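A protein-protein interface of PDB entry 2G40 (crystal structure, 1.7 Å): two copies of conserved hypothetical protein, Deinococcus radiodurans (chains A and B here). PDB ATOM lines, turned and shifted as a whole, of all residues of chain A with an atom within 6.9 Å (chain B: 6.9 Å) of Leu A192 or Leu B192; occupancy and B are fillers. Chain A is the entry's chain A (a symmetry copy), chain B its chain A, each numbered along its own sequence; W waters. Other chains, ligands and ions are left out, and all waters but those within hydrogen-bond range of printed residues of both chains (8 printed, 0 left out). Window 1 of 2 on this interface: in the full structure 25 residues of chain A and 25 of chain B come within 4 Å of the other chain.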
ATOM      1  N   ALA A 133      21.108  -1.086  29.002  1.00  0.00           N
ATOM      2  CA  ALA A 133      22.136  -1.238  27.985  1.00  0.00           C
ATOM      3  C   ALA A 133      21.722  -0.588  26.671  1.00  0.00           C
ATOM      4  O   ALA A 133      22.518   0.135  26.035  1.00  0.00           O
ATOM      5  CB  ALA A 133      22.473  -2.694  27.769  1.00  0.00           C
ATOM      6  N   ILE A 143      16.726  -3.578  27.211  1.00  0.00           N
ATOM      7  CA  ILE A 143      17.688  -4.615  27.549  1.00  0.00           C
ATOM      8  C   ILE A 143      18.616  -4.130  28.654  1.00  0.00           C
ATOM      9  O   ILE A 143      19.226  -3.056  28.553  1.00  0.00           O
ATOM     10  CB  ILE A 143      18.548  -5.015  26.358  1.00  0.00           C
ATOM     11  CG1 ILE A 143      17.676  -5.511  25.198  1.00  0.00           C
ATOM     12  CG2 ILE A 143      19.583  -6.106  26.801  1.00  0.00           C
ATOM     13  CD1 ILE A 143      18.425  -5.722  23.869  1.00  0.00           C
ATOM     14  N   LEU A 144      18.700  -4.939  29.694  1.00  0.00           N
ATOM     15  CA  LEU A 144      19.663  -4.776  30.743  1.00  0.00           C
ATOM     16  C   LEU A 144      20.781  -5.768  30.557  1.00  0.00           C
ATOM     17  O   LEU A 144      20.531  -6.955  30.311  1.00  0.00           O
ATOM     18  CB  LEU A 144      19.027  -5.060  32.093  1.00  0.00           C
ATOM     19  CG  LEU A 144      17.724  -4.348  32.460  1.00  0.00           C
ATOM     20  CD1 LEU A 144      17.483  -4.597  33.950  1.00  0.00           C
ATOM     21  CD2 LEU A 144      17.727  -2.856  32.152  1.00  0.00           C
ATOM     22  N   ASP A 145      22.002  -5.297  30.775  1.00  0.00           N
ATOM     23  CA  ASP A 145      23.172  -6.167  30.814  1.00  0.00           C
ATOM     24  C   ASP A 145      23.857  -6.178  32.183  1.00  0.00           C
ATOM     25  O   ASP A 145      24.928  -6.745  32.321  1.00  0.00           O
ATOM     26  CB  ASP A 145      24.166  -5.860  29.676  1.00  0.00           C
ATOM     27  CG  ASP A 145      24.856  -4.505  29.818  1.00  0.00           C
ATOM     28  OD1 ASP A 145      24.549  -3.749  30.756  1.00  0.00           O
ATOM     29  OD2 ASP A 145      25.684  -4.194  28.950  1.00  0.00           O
ATOM     30  N   HIS A 146      23.224  -5.557  33.176  1.00  0.00           N
ATOM     31  CA  HIS A 146      23.557  -5.753  34.588  1.00  0.00           C
ATOM     32  C   HIS A 146      24.933  -5.258  34.952  1.00  0.00           C
ATOM     33  O   HIS A 146      25.588  -5.796  35.822  1.00  0.00           O
ATOM     34  CB  HIS A 146      23.271  -7.216  34.937  1.00  0.00           C
ATOM     35  CG  HIS A 146      21.838  -7.564  34.698  1.00  0.00           C
ATOM     36  ND1 HIS A 146      20.825  -7.040  35.474  1.00  0.00           N
ATOM     37  CD2 HIS A 146      21.234  -8.274  33.717  1.00  0.00           C
ATOM     38  CE1 HIS A 146      19.663  -7.452  35.005  1.00  0.00           C
ATOM     39  NE2 HIS A 146      19.886  -8.218  33.954  1.00  0.00           N
ATOM     40  N   ARG A 153      20.760  -9.339  38.672  1.00  0.00           N
ATOM     41  CA  ARG A 153      19.443  -9.665  38.145  1.00  0.00           C
ATOM     42  C   ARG A 153      18.341  -9.536  39.189  1.00  0.00           C
ATOM     43  O   ARG A 153      17.254  -9.097  38.868  1.00  0.00           O
ATOM     44  CB  ARG A 153      19.474 -11.048  37.519  1.00  0.00           C
ATOM     45  CG  ARG A 153      20.293 -11.069  36.240  1.00  0.00           C
ATOM     46  CD  ARG A 153      19.886 -12.198  35.349  1.00  0.00           C
ATOM     47  NE  ARG A 153      20.523 -13.425  35.757  1.00  0.00           N
ATOM     48  CZ  ARG A 153      19.939 -14.624  35.816  1.00  0.00           C
ATOM     49  NH1 ARG A 153      18.652 -14.810  35.523  1.00  0.00           N
ATOM     50  NH2 ARG A 153      20.676 -15.655  36.196  1.00  0.00           N
ATOM     51  N   VAL A 179      20.647  -5.791  19.388  1.00  0.00           N
ATOM     52  CA  VAL A 179      21.544  -6.924  19.615  1.00  0.00           C
ATOM     53  C   VAL A 179      22.990  -6.540  19.332  1.00  0.00           C
ATOM     54  O   VAL A 179      23.899  -6.882  20.101  1.00  0.00           O
ATOM     55  CB  VAL A 179      21.128  -8.105  18.744  1.00  0.00           C
ATOM     56  CG1 VAL A 179      22.135  -9.230  18.834  1.00  0.00           C
ATOM     57  CG2 VAL A 179      19.755  -8.588  19.179  1.00  0.00           C
ATOM     58  N   VAL A 182      24.426  -4.797  22.271  1.00  0.00           N
ATOM     59  CA  VAL A 182      24.756  -5.624  23.439  1.00  0.00           C
ATOM     60  C   VAL A 182      25.635  -6.830  23.099  1.00  0.00           C
ATOM     61  O   VAL A 182      25.943  -7.629  23.974  1.00  0.00           O
ATOM     62  CB  VAL A 182      23.496  -6.099  24.189  1.00  0.00           C
ATOM     63  CG1 VAL A 182      22.748  -4.914  24.754  1.00  0.00           C
ATOM     64  CG2 VAL A 182      22.585  -6.937  23.305  1.00  0.00           C
ATOM     65  N   ALA A 183      26.035  -6.952  21.835  1.00  0.00           N
ATOM     66  CA  ALA A 183      26.878  -8.058  21.397  1.00  0.00           C
ATOM     67  C   ALA A 183      28.134  -8.197  22.259  1.00  0.00           C
ATOM     68  O   ALA A 183      28.527  -9.303  22.631  1.00  0.00           O
ATOM     69  CB  ALA A 183      27.264  -7.879  19.930  1.00  0.00           C
ATOM     70  N   SER A 185      28.682  -7.268  25.374  1.00  0.00           N
ATOM     71  CA  SER A 185      28.279  -7.781  26.688  1.00  0.00           C
ATOM     72  C   SER A 185      28.087  -9.288  26.630  1.00  0.00           C
ATOM     73  O   SER A 185      28.517 -10.006  27.526  1.00  0.00           O
ATOM     74  CB  SER A 185      26.990  -7.104  27.136  1.00  0.00           C
ATOM     75  OG  SER A 185      27.202  -5.727  27.323  1.00  0.00           O
ATOM     76  N   VAL A 186      27.475  -9.759  25.546  1.00  0.00           N
ATOM     77  CA  VAL A 186      27.221 -11.182  25.372  1.00  0.00           C
ATOM     78  C   VAL A 186      28.547 -11.906  25.244  1.00  0.00           C
ATOM     79  O   VAL A 186      28.764 -12.924  25.894  1.00  0.00           O
ATOM     80  CB  VAL A 186      26.309 -11.493  24.151  1.00  0.00           C
ATOM     81  CG1 VAL A 186      26.140 -12.988  23.978  1.00  0.00           C
ATOM     82  CG2 VAL A 186      24.955 -10.857  24.352  1.00  0.00           C
ATOM     83  N   GLY A 189      30.148 -12.503  28.446  1.00  0.00           N
ATOM     84  CA  GLY A 189      29.453 -13.407  29.331  1.00  0.00           C
ATOM     85  C   GLY A 189      28.491 -12.721  30.278  1.00  0.00           C
ATOM     86  O   GLY A 189      28.016 -13.345  31.246  1.00  0.00           O
ATOM     87  N   ARG A 190      28.163 -11.454  30.018  1.00  0.00           N
ATOM     88  CA  ARG A 190      27.233 -10.754  30.889  1.00  0.00           C
ATOM     89  C   ARG A 190      25.841 -11.256  30.578  1.00  0.00           C
ATOM     90  O   ARG A 190      25.500 -11.469  29.418  1.00  0.00           O
ATOM     91  CB  ARG A 190      27.255  -9.260  30.672  1.00  0.00           C
ATOM     92  CG  ARG A 190      28.553  -8.602  31.051  1.00  0.00           C
ATOM     93  CD  ARG A 190      28.465  -7.111  30.909  1.00  0.00           C
ATOM     94  NE  ARG A 190      29.786  -6.524  31.087  1.00  0.00           N
ATOM     95  CZ  ARG A 190      30.358  -6.290  32.262  1.00  0.00           C
ATOM     96  NH1 ARG A 190      29.736  -6.587  33.383  1.00  0.00           N
ATOM     97  NH2 ARG A 190      31.564  -5.737  32.310  1.00  0.00           N
ATOM     98  N   PRO A 191      25.028 -11.431  31.615  1.00  0.00           N
ATOM     99  CA  PRO A 191      23.641 -11.797  31.386  1.00  0.00           C
ATOM    100  C   PRO A 191      22.853 -10.655  30.798  1.00  0.00           C
ATOM    101  O   PRO A 191      23.141  -9.483  31.081  1.00  0.00           O
ATOM    102  CB  PRO A 191      23.130 -12.093  32.790  1.00  0.00           C
ATOM    103  CG  PRO A 191      24.011 -11.250  33.677  1.00  0.00           C
ATOM    104  CD  PRO A 191      25.336 -11.276  33.054  1.00  0.00           C
ATOM    105  N   LEU A 192      21.848 -10.994  30.004  1.00  0.00           N
ATOM    106  CA  LEU A 192      20.940  -9.975  29.476  1.00  0.00           C
ATOM    107  C   LEU A 192      19.541 -10.277  29.908  1.00  0.00           C
ATOM    108  O   LEU A 192      19.127 -11.437  29.931  1.00  0.00           O
ATOM    109  CB  LEU A 192      20.948  -9.920  27.959  1.00  0.00           C
ATOM    110  CG  LEU A 192      22.255  -9.751  27.203  1.00  0.00           C
ATOM    111  CD1 LEU A 192      21.914  -9.683  25.748  1.00  0.00           C
ATOM    112  CD2 LEU A 192      23.013  -8.515  27.613  1.00  0.00           C
ATOM    113  N   THR A 193      18.810  -9.220  30.217  1.00  0.00           N
ATOM    114  CA  THR A 193      17.409  -9.326  30.547  1.00  0.00           C
ATOM    115  C   THR A 193      16.689  -8.401  29.574  1.00  0.00           C
ATOM    116  O   THR A 193      16.958  -7.215  29.536  1.00  0.00           O
ATOM    117  CB  THR A 193      17.175  -8.917  32.007  1.00  0.00           C
ATOM    118  OG1 THR A 193      17.995  -9.728  32.871  1.00  0.00           O
ATOM    119  CG2 THR A 193      15.743  -9.037  32.354  1.00  0.00           C
ATOM    120  N   TRP A 194      15.802  -8.961  28.762  1.00  0.00           N
ATOM    121  CA  TRP A 194      15.056  -8.173  27.794  1.00  0.00           C
ATOM    122  C   TRP A 194      13.637  -8.037  28.297  1.00  0.00           C
ATOM    123  O   TRP A 194      12.924  -9.035  28.423  1.00  0.00           O
ATOM    124  CB  TRP A 194      14.964  -8.889  26.472  1.00  0.00           C
ATOM    125  CG  TRP A 194      16.222  -9.050  25.700  1.00  0.00           C
ATOM    126  CD1 TRP A 194      17.439  -9.412  26.166  1.00  0.00           C
ATOM    127  CD2 TRP A 194      16.357  -8.893  24.290  1.00  0.00           C
ATOM    128  NE1 TRP A 194      18.341  -9.471  25.134  1.00  0.00           N
ATOM    129  CE2 TRP A 194      17.700  -9.168  23.967  1.00  0.00           C
ATOM    130  CE3 TRP A 194      15.464  -8.566  23.258  1.00  0.00           C
ATOM    131  CZ2 TRP A 194      18.181  -9.100  22.662  1.00  0.00           C
ATOM    132  CZ3 TRP A 194      15.931  -8.494  21.980  1.00  0.00           C
ATOM    133  CH2 TRP A 194      17.282  -8.777  21.677  1.00  0.00           C
ATOM    134  N   LEU A 195      13.229  -6.802  28.540  1.00  0.00           N
ATOM    135  CA  LEU A 195      11.909  -6.475  29.049  1.00  0.00           C
ATOM    136  C   LEU A 195      11.188  -5.812  27.891  1.00  0.00           C
ATOM    137  O   LEU A 195      11.686  -4.838  27.371  1.00  0.00           O
ATOM    138  CB  LEU A 195      12.050  -5.496  30.209  1.00  0.00           C
ATOM    139  CG  LEU A 195      13.147  -5.872  31.210  1.00  0.00           C
ATOM    140  CD1 LEU A 195      13.524  -4.700  32.064  1.00  0.00           C
ATOM    141  CD2 LEU A 195      12.680  -7.035  32.049  1.00  0.00           C
ATOM    142  N   SER A 196      10.042  -6.346  27.473  1.00  0.00           N
ATOM    143  CA  SER A 196       9.417  -5.913  26.215  1.00  0.00           C
ATOM    144  C   SER A 196       7.925  -5.721  26.328  1.00  0.00           C
ATOM    145  O   SER A 196       7.228  -6.538  26.938  1.00  0.00           O
ATOM    146  CB  SER A 196       9.664  -6.920  25.084  1.00  0.00           C
ATOM    147  OG  SER A 196      11.043  -7.106  24.825  1.00  0.00           O
ATOM    148  N   ALA B 133      14.574 -21.403  24.940  1.00  0.00           N
ATOM    149  CA  ALA B 133      14.035 -20.951  23.668  1.00  0.00           C
ATOM    150  C   ALA B 133      14.976 -21.277  22.515  1.00  0.00           C
ATOM    151  O   ALA B 133      14.543 -21.778  21.455  1.00  0.00           O
ATOM    152  CB  ALA B 133      13.738 -19.471  23.701  1.00  0.00           C
ATOM    153  N   ILE B 143      19.168 -18.781  25.739  1.00  0.00           N
ATOM    154  CA  ILE B 143      18.098 -17.810  25.905  1.00  0.00           C
ATOM    155  C   ILE B 143      16.831 -18.504  26.386  1.00  0.00           C
ATOM    156  O   ILE B 143      16.371 -19.485  25.787  1.00  0.00           O
ATOM    157  CB  ILE B 143      17.769 -17.084  24.609  1.00  0.00           C
ATOM    158  CG1 ILE B 143      19.007 -16.364  24.059  1.00  0.00           C
ATOM    159  CG2 ILE B 143      16.587 -16.083  24.852  1.00  0.00           C
ATOM    160  CD1 ILE B 143      18.846 -15.792  22.638  1.00  0.00           C
ATOM    161  N   LEU B 144      16.293 -17.973  27.470  1.00  0.00           N
ATOM    162  CA  LEU B 144      14.999 -18.338  27.967  1.00  0.00           C
ATOM    163  C   LEU B 144      14.000 -17.274  27.598  1.00  0.00           C
ATOM    164  O   LEU B 144      14.265 -16.077  27.775  1.00  0.00           O
ATOM    165  CB  LEU B 144      15.022 -18.430  29.483  1.00  0.00           C
ATOM    166  CG  LEU B 144      16.104 -19.278  30.155  1.00  0.00           C
ATOM    167  CD1 LEU B 144      15.712 -19.418  31.627  1.00  0.00           C
ATOM    168  CD2 LEU B 144      16.304 -20.647  29.514  1.00  0.00           C
ATOM    169  N   ASP B 145      12.821 -17.719  27.183  1.00  0.00           N
ATOM    170  CA  ASP B 145      11.690 -16.825  26.961  1.00  0.00           C
ATOM    171  C   ASP B 145      10.513 -17.116  27.896  1.00  0.00           C
ATOM    172  O   ASP B 145       9.449 -16.545  27.726  1.00  0.00           O
ATOM    173  CB  ASP B 145      11.256 -16.789  25.482  1.00  0.00           C
ATOM    174  CG  ASP B 145      10.639 -18.098  24.996  1.00  0.00           C
ATOM    175  OD1 ASP B 145      10.582 -19.078  25.760  1.00  0.00           O
ATOM    176  OD2 ASP B 145      10.248 -18.142  23.820  1.00  0.00           O
ATOM    177  N   HIS B 146      10.724 -17.995  28.872  1.00  0.00           N
ATOM    178  CA  HIS B 146       9.842 -18.137  30.031  1.00  0.00           C
ATOM    179  C   HIS B 146       8.464 -18.633  29.677  1.00  0.00           C
ATOM    180  O   HIS B 146       7.487 -18.292  30.314  1.00  0.00           O
ATOM    181  CB  HIS B 146       9.886 -16.822  30.815  1.00  0.00           C
ATOM    182  CG  HIS B 146      11.273 -16.503  31.267  1.00  0.00           C
ATOM    183  ND1 HIS B 146      11.914 -17.255  32.229  1.00  0.00           N
ATOM    184  CD2 HIS B 146      12.182 -15.605  30.820  1.00  0.00           C
ATOM    185  CE1 HIS B 146      13.144 -16.801  32.385  1.00  0.00           C
ATOM    186  NE2 HIS B 146      13.322 -15.788  31.558  1.00  0.00           N
ATOM    187  N   ARG B 153      10.566 -15.823  35.642  1.00  0.00           N
ATOM    188  CA  ARG B 153      11.965 -15.446  35.788  1.00  0.00           C
ATOM    189  C   ARG B 153      12.560 -15.887  37.120  1.00  0.00           C
ATOM    190  O   ARG B 153      13.705 -16.290  37.166  1.00  0.00           O
ATOM    191  CB  ARG B 153      12.116 -13.952  35.566  1.00  0.00           C
ATOM    192  CG  ARG B 153      11.881 -13.573  34.113  1.00  0.00           C
ATOM    193  CD  ARG B 153      12.551 -12.282  33.770  1.00  0.00           C
ATOM    194  NE  ARG B 153      11.740 -11.162  34.177  1.00  0.00           N
ATOM    195  CZ  ARG B 153      12.186 -10.047  34.760  1.00  0.00           C
ATOM    196  NH1 ARG B 153      13.471  -9.863  35.064  1.00  0.00           N
ATOM    197  NH2 ARG B 153      11.305  -9.104  35.052  1.00  0.00           N
ATOM    198  N   VAL B 179      18.613 -14.502  17.810  1.00  0.00           N
ATOM    199  CA  VAL B 179      17.643 -13.414  17.930  1.00  0.00           C
ATOM    200  C   VAL B 179      16.455 -13.640  17.003  1.00  0.00           C
ATOM    201  O   VAL B 179      15.297 -13.450  17.400  1.00  0.00           O
ATOM    202  CB  VAL B 179      18.311 -12.079  17.620  1.00  0.00           C
ATOM    203  CG1 VAL B 179      17.295 -10.959  17.573  1.00  0.00           C
ATOM    204  CG2 VAL B 179      19.366 -11.790  18.676  1.00  0.00           C
ATOM    205  N   VAL B 182      14.052 -15.975  18.587  1.00  0.00           N
ATOM    206  CA  VAL B 182      13.237 -15.446  19.688  1.00  0.00           C
ATOM    207  C   VAL B 182      12.507 -14.150  19.333  1.00  0.00           C
ATOM    208  O   VAL B 182      11.831 -13.576  20.177  1.00  0.00           O
ATOM    209  CB  VAL B 182      14.063 -15.239  20.974  1.00  0.00           C
ATOM    210  CG1 VAL B 182      14.581 -16.564  21.480  1.00  0.00           C
ATOM    211  CG2 VAL B 182      15.206 -14.258  20.768  1.00  0.00           C
ATOM    212  N   ALA B 183      12.643 -13.698  18.087  1.00  0.00           N
ATOM    213  CA  ALA B 183      11.990 -12.475  17.635  1.00  0.00           C
ATOM    214  C   ALA B 183      10.489 -12.487  17.924  1.00  0.00           C
ATOM    215  O   ALA B 183       9.922 -11.488  18.367  1.00  0.00           O
ATOM    216  CB  ALA B 183      12.238 -12.266  16.142  1.00  0.00           C
ATOM    217  N   SER B 185       8.784 -14.126  20.221  1.00  0.00           N
ATOM    218  CA  SER B 185       8.597 -13.976  21.668  1.00  0.00           C
ATOM    219  C   SER B 185       8.716 -12.513  22.066  1.00  0.00           C
ATOM    220  O   SER B 185       7.925 -12.017  22.861  1.00  0.00           O
ATOM    221  CB  SER B 185       9.631 -14.809  22.414  1.00  0.00           C
ATOM    222  OG  SER B 185       9.434 -16.177  22.154  1.00  0.00           O
ATOM    223  N   VAL B 186       9.687 -11.822  21.473  1.00  0.00           N
ATOM    224  CA  VAL B 186       9.914 -10.416  21.773  1.00  0.00           C
ATOM    225  C   VAL B 186       8.715  -9.613  21.305  1.00  0.00           C
ATOM    226  O   VAL B 186       8.201  -8.777  22.042  1.00  0.00           O
ATOM    227  CB  VAL B 186      11.222  -9.862  21.140  1.00  0.00           C
ATOM    228  CG1 VAL B 186      11.368  -8.381  21.424  1.00  0.00           C
ATOM    229  CG2 VAL B 186      12.412 -10.597  21.705  1.00  0.00           C
ATOM    230  N   GLY B 189       5.932  -9.741  23.631  1.00  0.00           N
ATOM    231  CA  GLY B 189       6.163  -9.122  24.915  1.00  0.00           C
ATOM    232  C   GLY B 189       6.698 -10.071  25.967  1.00  0.00           C
ATOM    233  O   GLY B 189       6.710  -9.731  27.166  1.00  0.00           O
ATOM    234  N   ARG B 190       7.169 -11.250  25.557  1.00  0.00           N
ATOM    235  CA  ARG B 190       7.706 -12.191  26.527  1.00  0.00           C
ATOM    236  C   ARG B 190       9.077 -11.702  26.936  1.00  0.00           C
ATOM    237  O   ARG B 190       9.844 -11.227  26.103  1.00  0.00           O
ATOM    238  CB  ARG B 190       7.852 -13.582  25.957  1.00  0.00           C
ATOM    239  CG  ARG B 190       6.547 -14.244  25.607  1.00  0.00           C
ATOM    240  CD  ARG B 190       6.764 -15.656  25.150  1.00  0.00           C
ATOM    241  NE  ARG B 190       5.516 -16.198  24.630  1.00  0.00           N
ATOM    242  CZ  ARG B 190       4.533 -16.684  25.378  1.00  0.00           C
ATOM    243  NH1 ARG B 190       4.635 -16.707  26.690  1.00  0.00           N
ATOM    244  NH2 ARG B 190       3.441 -17.167  24.799  1.00  0.00           N
ATOM    245  N   PRO B 191       9.394 -11.832  28.220  1.00  0.00           N
ATOM    246  CA  PRO B 191      10.734 -11.494  28.666  1.00  0.00           C
ATOM    247  C   PRO B 191      11.751 -12.495  28.183  1.00  0.00           C
ATOM    248  O   PRO B 191      11.436 -13.684  28.028  1.00  0.00           O
ATOM    249  CB  PRO B 191      10.621 -11.580  30.183  1.00  0.00           C
ATOM    250  CG  PRO B 191       9.504 -12.569  30.403  1.00  0.00           C
ATOM    251  CD  PRO B 191       8.541 -12.320  29.327  1.00  0.00           C
ATOM    252  N   LEU B 192      12.971 -12.025  27.971  1.00  0.00           N
ATOM    253  CA  LEU B 192      14.068 -12.927  27.620  1.00  0.00           C
ATOM    254  C   LEU B 192      15.156 -12.816  28.637  1.00  0.00           C
ATOM    255  O   LEU B 192      15.465 -11.721  29.111  1.00  0.00           O
ATOM    256  CB  LEU B 192      14.673 -12.606  26.266  1.00  0.00           C
ATOM    257  CG  LEU B 192      13.791 -12.514  25.031  1.00  0.00           C
ATOM    258  CD1 LEU B 192      14.692 -12.239  23.868  1.00  0.00           C
ATOM    259  CD2 LEU B 192      12.999 -13.772  24.782  1.00  0.00           C
ATOM    260  N   THR B 193      15.756 -13.954  28.943  1.00  0.00           N
ATOM    261  CA  THR B 193      16.898 -14.007  29.824  1.00  0.00           C
ATOM    262  C   THR B 193      17.997 -14.699  29.028  1.00  0.00           C
ATOM    263  O   THR B 193      17.828 -15.824  28.593  1.00  0.00           O
ATOM    264  CB  THR B 193      16.547 -14.775  31.104  1.00  0.00           C
ATOM    265  OG1 THR B 193      15.407 -14.160  31.736  1.00  0.00           O
ATOM    266  CG2 THR B 193      17.709 -14.820  32.016  1.00  0.00           C
ATOM    267  N   TRP B 194      19.104 -14.004  28.807  1.00  0.00           N
ATOM    268  CA  TRP B 194      20.217 -14.566  28.059  1.00  0.00           C
ATOM    269  C   TRP B 194      21.319 -14.897  29.039  1.00  0.00           C
ATOM    270  O   TRP B 194      21.867 -14.001  29.684  1.00  0.00           O
ATOM    271  CB  TRP B 194      20.796 -13.552  27.107  1.00  0.00           C
ATOM    272  CG  TRP B 194      19.947 -13.140  25.960  1.00  0.00           C
ATOM    273  CD1 TRP B 194      18.628 -12.840  25.971  1.00  0.00           C
ATOM    274  CD2 TRP B 194      20.399 -12.936  24.624  1.00  0.00           C
ATOM    275  NE1 TRP B 194      18.216 -12.481  24.713  1.00  0.00           N
ATOM    276  CE2 TRP B 194      19.287 -12.520  23.866  1.00  0.00           C
ATOM    277  CE3 TRP B 194      21.648 -13.045  23.993  1.00  0.00           C
ATOM    278  CZ2 TRP B 194      19.376 -12.238  22.506  1.00  0.00           C
ATOM    279  CZ3 TRP B 194      21.739 -12.775  22.660  1.00  0.00           C
ATOM    280  CH2 TRP B 194      20.611 -12.355  21.920  1.00  0.00           C
ATOM    281  N   LEU B 195      21.660 -16.174  29.113  1.00  0.00           N
ATOM    282  CA  LEU B 195      22.678 -16.685  30.012  1.00  0.00           C
ATOM    283  C   LEU B 195      23.838 -17.079  29.117  1.00  0.00           C
ATOM    284  O   LEU B 195      23.644 -17.867  28.218  1.00  0.00           O
ATOM    285  CB  LEU B 195      22.134 -17.912  30.736  1.00  0.00           C
ATOM    286  CG  LEU B 195      20.709 -17.737  31.270  1.00  0.00           C
ATOM    287  CD1 LEU B 195      20.083 -19.062  31.582  1.00  0.00           C
ATOM    288  CD2 LEU B 195      20.738 -16.844  32.485  1.00  0.00           C
ATOM    289  N   SER B 196      25.025 -16.519  29.341  1.00  0.00           N
ATOM    290  CA  SER B 196      26.125 -16.661  28.377  1.00  0.00           C
ATOM    291  C   SER B 196      27.454 -16.953  29.029  1.00  0.00           C
ATOM    292  O   SER B 196      27.802 -16.350  30.049  1.00  0.00           O
ATOM    293  CB  SER B 196      26.302 -15.394  27.528  1.00  0.00           C
ATOM    294  OG  SER B 196      25.135 -15.078  26.792  1.00  0.00           O
HETATM  295  O   HOH W   1      15.430 -16.127  35.333  1.00  0.00           O
HETATM  296  O   HOH W   2      25.473 -14.716  31.443  1.00  0.00           O
HETATM  297  O   HOH W   3       5.454  -7.788  28.404  1.00  0.00           O
HETATM  298  O   HOH W   4      16.423  -8.711  36.518  1.00  0.00           O
HETATM  299  O   HOH W   5      11.735  -9.334  25.869  1.00  0.00           O
HETATM  300  O   HOH W   6      23.966 -13.144  27.983  1.00  0.00           O
HETATM  301  O   HOH W   7       8.882  -8.587  28.701  1.00  0.00           O
HETATM  302  O   HOH W   8      28.769 -15.597  32.363  1.00  0.00           O
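Val B179 touches its own counterpart, Val A179. Val A186 touches Trp B194, and with the chains exchanged Trp A194 touches Val B186. Leu A192 touches its own counterpart, Leu B192. Trp A194 touches its own counterpart, Trp B194. Positions printed for both chains: 133, 143, 144, 145, 146, 153, 179, 182, 183, 185, 186, 189, 190, 191, 192, 193, 194, 195 and 196. Of the 19 pairs that touch across the chains among the printed residues, 19 have their exchanged pair printed and touching as well.
Water W1 lies within hydrogen-bond range of the backbone carbonyl oxygen of Arg B153 (2.5 Å) and the guanidinium group of Arg A153 (3.5 Å). Water W4 bridges the backbone carbonyl oxygen (O) of Arg A153 (2.5 Å) and the guanidinium group (NH1) of Arg B153 (3.5 Å). Water W5 lies within hydrogen-bond range of OG of Ser A196, O of Arg B190 and O of Trp A194. Water W8 bridges O of Ser B196 and O of Gly A189. Water W2 lies within hydrogen-bond range of N of Ser B196 (2.8 Å) and O of Gly A189 (2.9 Å). Water W7 lies within hydrogen-bond range of N of Ser A196 (2.8 Å) and O of Gly B189 (2.9 Å).
O of Leu B192 lies within hydrogen-bond range of N of Trp A194. The backbone NH of Trp B194 is in hydrogen-bond range of the backbone carbonyl oxygen of Leu A192 (2.8 Å). O of Gly A189 sits close to O of Ser B196 (3.2 Å). The indole nitrogen of Trp A194 sits close to the indole nitrogen of Trp B194 (3.0 Å). The backbone carbonyl oxygen of Ser A196 sits close to the backbone carbonyl oxygen of Gly B189, 3.2 Å away.
Arg A153 touches Leu B195 (NH2 to CD2, 3.9 Å). Val B179 touches Val A179 (CG2 to CG2, 3.3 Å). Val A186 touches Trp B194. CG1 of Val A186 touches OG of Ser B196, at 3.6 Å. CA of Pro A191 touches O of Trp B194, at 3.3 Å. Leu B192 touches Leu A192 (O to O, 3.8 Å). Leu A192 touches Thr B193. Arg B153 touches Thr A193. CE3 of Trp A194 touches CG2 of Val B186 (3.98 Å). Pro B191 touches Trp A194 (CA to O, 3.3 Å).
Of the printed residues of chain B, Leu A192 touches Leu B192, Thr B193 and Trp B194. Printed residues of chain B within 4 Å of Ser A196: Val B186 (3.6 Å) and Gly B189 (3.2 Å). Of the printed residues of chain A, Thr B193 touches Arg A153 (3.6 Å) and Leu A192 (3.4 Å). Of the printed residues of chain A, Gly B189 touches Ser A196 (3.2 Å). Printed residues of chain B within 4 Å of Arg A153: Thr B193 (3.6 Å) and Leu B195 (3.9 Å). The nearest residue of chain B that does not touch Leu A192 is Leu B195 (5.3 Å). The nearest printed residue of chain A that does not touch Trp B194 is Arg A190 (4.4 Å).
The backbone carbonyl oxygen of Leu B144 is in hydrogen-bond range of the backbone NH of Thr B193. The side-chain hydroxyl of Thr B193 sits at hydrogen-bond distance from a ring nitrogen (NE2) of His B146 (2.7 Å). The backbone carbonyl oxygen of Leu A144 sits at hydrogen-bond distance from the backbone NH of Thr A193, 2.8 Å away. A ring nitrogen (NE2) of His A146 lies within hydrogen-bond range of the side-chain hydroxyl of Thr A193 (2.7 Å).
Hydrophobic or aromatic side chains of chain B within 4 Å of the printed part of chain A: Val B179, Val B186, Pro B191, Leu B192, Trp B194 and Leu B195. Of the 19 printed residues of chain A, 10 touch a printed residue of chain B. Hydrophobic or aromatic side chains of chain A within 4 Å of the printed part of chain B: Val A179, Val A186, Pro A191, Leu A192, Trp A194 and Leu A195.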
